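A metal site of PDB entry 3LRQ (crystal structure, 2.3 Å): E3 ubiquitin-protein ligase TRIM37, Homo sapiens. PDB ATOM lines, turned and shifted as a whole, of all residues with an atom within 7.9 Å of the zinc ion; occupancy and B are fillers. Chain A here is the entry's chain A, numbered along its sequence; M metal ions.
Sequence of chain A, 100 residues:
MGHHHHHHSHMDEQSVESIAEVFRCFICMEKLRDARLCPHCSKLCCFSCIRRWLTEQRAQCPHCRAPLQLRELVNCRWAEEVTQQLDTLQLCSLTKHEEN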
ATOM      1  N   LEU A  37      -4.211 -35.119  -4.749  1.00  0.00           N
ATOM      2  CA  LEU A  37      -3.153 -34.466  -4.041  1.00  0.00           C
ATOM      3  C   LEU A  37      -2.025 -34.129  -5.024  1.00  0.00           C
ATOM      4  O   LEU A  37      -1.643 -34.965  -5.842  1.00  0.00           O
ATOM      5  CB  LEU A  37      -2.688 -35.397  -2.928  1.00  0.00           C
ATOM      6  CG  LEU A  37      -1.541 -34.972  -2.044  1.00  0.00           C
ATOM      7  CD1 LEU A  37      -1.905 -35.123  -0.547  1.00  0.00           C
ATOM      8  CD2 LEU A  37      -0.316 -35.788  -2.425  1.00  0.00           C
ATOM      9  N   CYS A  38      -1.535 -32.897  -4.964  1.00  0.00           N
ATOM     10  CA  CYS A  38      -0.366 -32.510  -5.749  1.00  0.00           C
ATOM     11  C   CYS A  38       0.891 -33.140  -5.166  1.00  0.00           C
ATOM     12  O   CYS A  38       1.211 -32.931  -3.999  1.00  0.00           O
ATOM     13  CB  CYS A  38      -0.170 -30.992  -5.709  1.00  0.00           C
ATOM     14  SG  CYS A  38       1.426 -30.537  -6.465  1.00  0.00           S
ATOM     15  N   PRO A  39       1.619 -33.902  -5.997  1.00  0.00           N
ATOM     16  CA  PRO A  39       2.776 -34.694  -5.577  1.00  0.00           C
ATOM     17  C   PRO A  39       3.915 -33.819  -5.089  1.00  0.00           C
ATOM     18  O   PRO A  39       4.750 -34.289  -4.317  1.00  0.00           O
ATOM     19  CB  PRO A  39       3.219 -35.393  -6.875  1.00  0.00           C
ATOM     20  CG  PRO A  39       2.130 -35.164  -7.860  1.00  0.00           C
ATOM     21  CD  PRO A  39       1.424 -33.916  -7.447  1.00  0.00           C
ATOM     22  N   HIS A  40       3.948 -32.568  -5.516  1.00  0.00           N
ATOM     23  CA  HIS A  40       5.093 -31.717  -5.225  1.00  0.00           C
ATOM     24  C   HIS A  40       4.936 -30.922  -3.948  1.00  0.00           C
ATOM     25  O   HIS A  40       5.934 -30.573  -3.326  1.00  0.00           O
ATOM     26  CB  HIS A  40       5.372 -30.756  -6.382  1.00  0.00           C
ATOM     27  CG  HIS A  40       5.419 -31.428  -7.716  1.00  0.00           C
ATOM     28  ND1 HIS A  40       6.350 -32.405  -8.016  1.00  0.00           N
ATOM     29  CD2 HIS A  40       4.632 -31.300  -8.805  1.00  0.00           C
ATOM     30  CE1 HIS A  40       6.145 -32.820  -9.253  1.00  0.00           C
ATOM     31  NE2 HIS A  40       5.108 -32.164  -9.756  1.00  0.00           N
ATOM     32  N   CYS A  41       3.703 -30.578  -3.598  1.00  0.00           N
ATOM     33  CA  CYS A  41       3.490 -29.738  -2.420  1.00  0.00           C
ATOM     34  C   CYS A  41       2.470 -30.325  -1.441  1.00  0.00           C
ATOM     35  O   CYS A  41       2.301 -29.810  -0.332  1.00  0.00           O
ATOM     36  CB  CYS A  41       3.092 -28.316  -2.852  1.00  0.00           C
ATOM     37  SG  CYS A  41       1.351 -28.115  -3.371  1.00  0.00           S
ATOM     38  N   SER A  42       1.767 -31.365  -1.882  1.00  0.00           N
ATOM     39  CA  SER A  42       0.753 -32.112  -1.109  1.00  0.00           C
ATOM     40  C   SER A  42      -0.584 -31.383  -0.859  1.00  0.00           C
ATOM     41  O   SER A  42      -1.428 -31.861  -0.095  1.00  0.00           O
ATOM     42  CB  SER A  42       1.315 -32.665   0.220  1.00  0.00           C
ATOM     43  OG  SER A  42       1.466 -31.655   1.211  1.00  0.00           O
ATOM     44  N   LYS A  43      -0.788 -30.242  -1.504  1.00  0.00           N
ATOM     45  CA  LYS A  43      -2.111 -29.622  -1.457  1.00  0.00           C
ATOM     46  C   LYS A  43      -3.138 -30.541  -2.071  1.00  0.00           C
ATOM     47  O   LYS A  43      -2.875 -31.208  -3.068  1.00  0.00           O
ATOM     48  CB  LYS A  43      -2.123 -28.268  -2.142  1.00  0.00           C
ATOM     49  CG  LYS A  43      -1.539 -27.159  -1.293  1.00  0.00           C
ATOM     50  CD  LYS A  43      -2.303 -26.979   0.016  1.00  0.00           C
ATOM     51  CE  LYS A  43      -1.713 -25.763   0.775  1.00  0.00           C
ATOM     52  NZ  LYS A  43      -2.549 -25.293   1.911  1.00  0.00           N
ATOM     53  N   LEU A  44      -4.327 -30.557  -1.463  1.00  0.00           N
ATOM     54  CA  LEU A  44      -5.438 -31.382  -1.921  1.00  0.00           C
ATOM     55  C   LEU A  44      -6.476 -30.536  -2.675  1.00  0.00           C
ATOM     56  O   LEU A  44      -6.774 -29.422  -2.261  1.00  0.00           O
ATOM     57  CB  LEU A  44      -6.105 -32.067  -0.725  1.00  0.00           C
ATOM     58  CG  LEU A  44      -5.309 -33.121   0.070  1.00  0.00           C
ATOM     59  CD1 LEU A  44      -5.342 -32.829   1.553  1.00  0.00           C
ATOM     60  CD2 LEU A  44      -5.802 -34.565  -0.201  1.00  0.00           C
ATOM     61  N   GLN A  60      -0.273 -26.222 -14.179  1.00  0.00           N
ATOM     62  CA  GLN A  60       0.512 -26.086 -12.960  1.00  0.00           C
ATOM     63  C   GLN A  60      -0.351 -26.171 -11.713  1.00  0.00           C
ATOM     64  O   GLN A  60      -1.544 -25.840 -11.747  1.00  0.00           O
ATOM     65  CB  GLN A  60       1.258 -24.739 -12.957  1.00  0.00           C
ATOM     66  CG  GLN A  60       2.200 -24.573 -14.134  1.00  0.00           C
ATOM     67  CD  GLN A  60       2.682 -23.142 -14.316  1.00  0.00           C
ATOM     68  OE1 GLN A  60       2.651 -22.342 -13.389  1.00  0.00           O
ATOM     69  NE2 GLN A  60       3.135 -22.815 -15.510  1.00  0.00           N
ATOM     70  N   CYS A  61       0.264 -26.574 -10.603  1.00  0.00           N
ATOM     71  CA  CYS A  61      -0.438 -26.684  -9.347  1.00  0.00           C
ATOM     72  C   CYS A  61      -0.950 -25.295  -8.983  1.00  0.00           C
ATOM     73  O   CYS A  61      -0.204 -24.324  -9.067  1.00  0.00           O
ATOM     74  CB  CYS A  61       0.490 -27.193  -8.242  1.00  0.00           C
ATOM     75  SG  CYS A  61      -0.374 -27.233  -6.654  1.00  0.00           S
ATOM     76  N   PRO A  62      -2.228 -25.187  -8.587  1.00  0.00           N
ATOM     77  CA  PRO A  62      -2.772 -23.854  -8.292  1.00  0.00           C
ATOM     78  C   PRO A  62      -2.098 -23.269  -7.053  1.00  0.00           C
ATOM     79  O   PRO A  62      -2.080 -22.061  -6.922  1.00  0.00           O
ATOM     80  CB  PRO A  62      -4.263 -24.129  -8.032  1.00  0.00           C
ATOM     81  CG  PRO A  62      -4.272 -25.506  -7.479  1.00  0.00           C
ATOM     82  CD  PRO A  62      -3.269 -26.228  -8.406  1.00  0.00           C
ATOM     83  N   HIS A  63      -1.551 -24.101  -6.180  1.00  0.00           N
ATOM     84  CA  HIS A  63      -0.862 -23.592  -5.004  1.00  0.00           C
ATOM     85  C   HIS A  63       0.622 -23.417  -5.224  1.00  0.00           C
ATOM     86  O   HIS A  63       1.161 -22.346  -4.979  1.00  0.00           O
ATOM     87  CB  HIS A  63      -1.086 -24.494  -3.795  1.00  0.00           C
ATOM     88  CG  HIS A  63      -0.207 -24.173  -2.618  1.00  0.00           C
ATOM     89  ND1 HIS A  63       0.788 -25.021  -2.189  1.00  0.00           N
ATOM     90  CD2 HIS A  63      -0.193 -23.114  -1.767  1.00  0.00           C
ATOM     91  CE1 HIS A  63       1.388 -24.500  -1.128  1.00  0.00           C
ATOM     92  NE2 HIS A  63       0.807 -23.349  -0.850  1.00  0.00           N
ATOM     93  N   CYS A  64       1.309 -24.459  -5.660  1.00  0.00           N
ATOM     94  CA  CYS A  64       2.760 -24.385  -5.626  1.00  0.00           C
ATOM     95  C   CYS A  64       3.324 -24.003  -6.981  1.00  0.00           C
ATOM     96  O   CYS A  64       4.511 -23.740  -7.095  1.00  0.00           O
ATOM     97  CB  CYS A  64       3.381 -25.691  -5.127  1.00  0.00           C
ATOM     98  SG  CYS A  64       3.468 -26.994  -6.373  1.00  0.00           S
ATOM     99  N   ARG A  65       2.468 -24.029  -8.006  1.00  0.00           N
ATOM    100  CA  ARG A  65       2.827 -23.578  -9.352  1.00  0.00           C
ATOM    101  C   ARG A  65       3.729 -24.526 -10.154  1.00  0.00           C
ATOM    102  O   ARG A  65       4.033 -24.253 -11.321  1.00  0.00           O
ATOM    103  CB  ARG A  65       3.449 -22.181  -9.321  1.00  0.00           C
ATOM    104  CG  ARG A  65       2.495 -21.084  -8.845  1.00  0.00           C
ATOM    105  CD  ARG A  65       3.084 -19.701  -9.111  1.00  0.00           C
ATOM    106  NE  ARG A  65       2.201 -18.629  -8.680  1.00  0.00           N
ATOM    107  CZ  ARG A  65       2.368 -17.333  -8.987  1.00  0.00           C
ATOM    108  NH1 ARG A  65       3.391 -16.945  -9.748  1.00  0.00           N
ATOM    109  NH2 ARG A  65       1.497 -16.430  -8.537  1.00  0.00           N
ATOM    110  N   ALA A  66       4.135 -25.641  -9.537  1.00  0.00           N
ATOM    111  CA  ALA A  66       4.918 -26.646 -10.255  1.00  0.00           C
ATOM    112  C   ALA A  66       4.172 -27.183 -11.481  1.00  0.00           C
ATOM    113  O   ALA A  66       2.952 -27.375 -11.430  1.00  0.00           O
ATOM    114  CB  ALA A  66       5.294 -27.797  -9.300  1.00  0.00           C
ATOM    115  N   PRO A  67       4.889 -27.408 -12.594  1.00  0.00           N
ATOM    116  CA  PRO A  67       4.274 -28.095 -13.723  1.00  0.00           C
ATOM    117  C   PRO A  67       3.581 -29.328 -13.216  1.00  0.00           C
ATOM    118  O   PRO A  67       4.065 -29.938 -12.251  1.00  0.00           O
ATOM    119  CB  PRO A  67       5.463 -28.472 -14.606  1.00  0.00           C
ATOM    120  CG  PRO A  67       6.436 -27.381 -14.348  1.00  0.00           C
ATOM    121  CD  PRO A  67       6.278 -26.995 -12.897  1.00  0.00           C
ATOM    122  N   LEU A  68       2.471 -29.694 -13.838  1.00  0.00           N
ATOM    123  CA  LEU A  68       1.628 -30.735 -13.294  1.00  0.00           C
ATOM    124  C   LEU A  68       0.647 -31.170 -14.360  1.00  0.00           C
ATOM    125  O   LEU A  68      -0.025 -30.334 -14.964  1.00  0.00           O
ATOM    126  CB  LEU A  68       0.867 -30.204 -12.065  1.00  0.00           C
ATOM    127  CG  LEU A  68       0.108 -31.233 -11.239  1.00  0.00           C
ATOM    128  CD1 LEU A  68       1.103 -32.131 -10.503  1.00  0.00           C
ATOM    129  CD2 LEU A  68      -0.867 -30.570 -10.254  1.00  0.00           C
ATOM    130  N   LEU A  73      -1.229 -36.478 -10.610  1.00  0.00           N
ATOM    131  CA  LEU A  73      -1.979 -36.252  -9.373  1.00  0.00           C
ATOM    132  C   LEU A  73      -2.166 -37.544  -8.605  1.00  0.00           C
ATOM    133  O   LEU A  73      -2.403 -38.592  -9.198  1.00  0.00           O
ATOM    134  CB  LEU A  73      -3.344 -35.643  -9.684  1.00  0.00           C
ATOM    135  CG  LEU A  73      -3.369 -34.183 -10.099  1.00  0.00           C
ATOM    136  CD1 LEU A  73      -4.668 -33.940 -10.809  1.00  0.00           C
ATOM    137  CD2 LEU A  73      -3.219 -33.274  -8.895  1.00  0.00           C
HETATM  138 ZN    ZN M   1       1.528 -28.234  -5.634  1.00  0.00          ZN
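Within 4 Å of the zinc ion: Cys 38, Cys 41, Cys 61 and Cys 64. Along chain A the residues within 4 Å of the zinc ion span positions 38 to 64.
The zinc ion is bound by SG of Cys 41 (2.3 Å), SG of Cys 61 (2.4 Å), SG of Cys 64 (2.4 Å) and SG of Cys 38 (2.5 Å).
N of Cys 38 lies within hydrogen-bond range of O of Lys 43 (2.9 Å). The backbone NH (N) of Cys 61 is in hydrogen-bond range of the backbone carbonyl oxygen (O) of Ala 66 (2.9 Å). The side-chain sulfur of Cys 38 sits close to the backbone NH of His 40. The side-chain sulfur (SG) of Cys 41 sits close to the backbone NH (N) of Lys 43 (3.5 Å). The side-chain sulfur of Cys 41 sits close to a ring nitrogen (ND1) of His 63. The backbone NH (N) of His 63 sits close to the side-chain sulfur (SG) of Cys 61 (3.4 Å). The backbone NH of Ala 66 lies close to the side-chain sulfur of Cys 64, 3.5 Å away.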
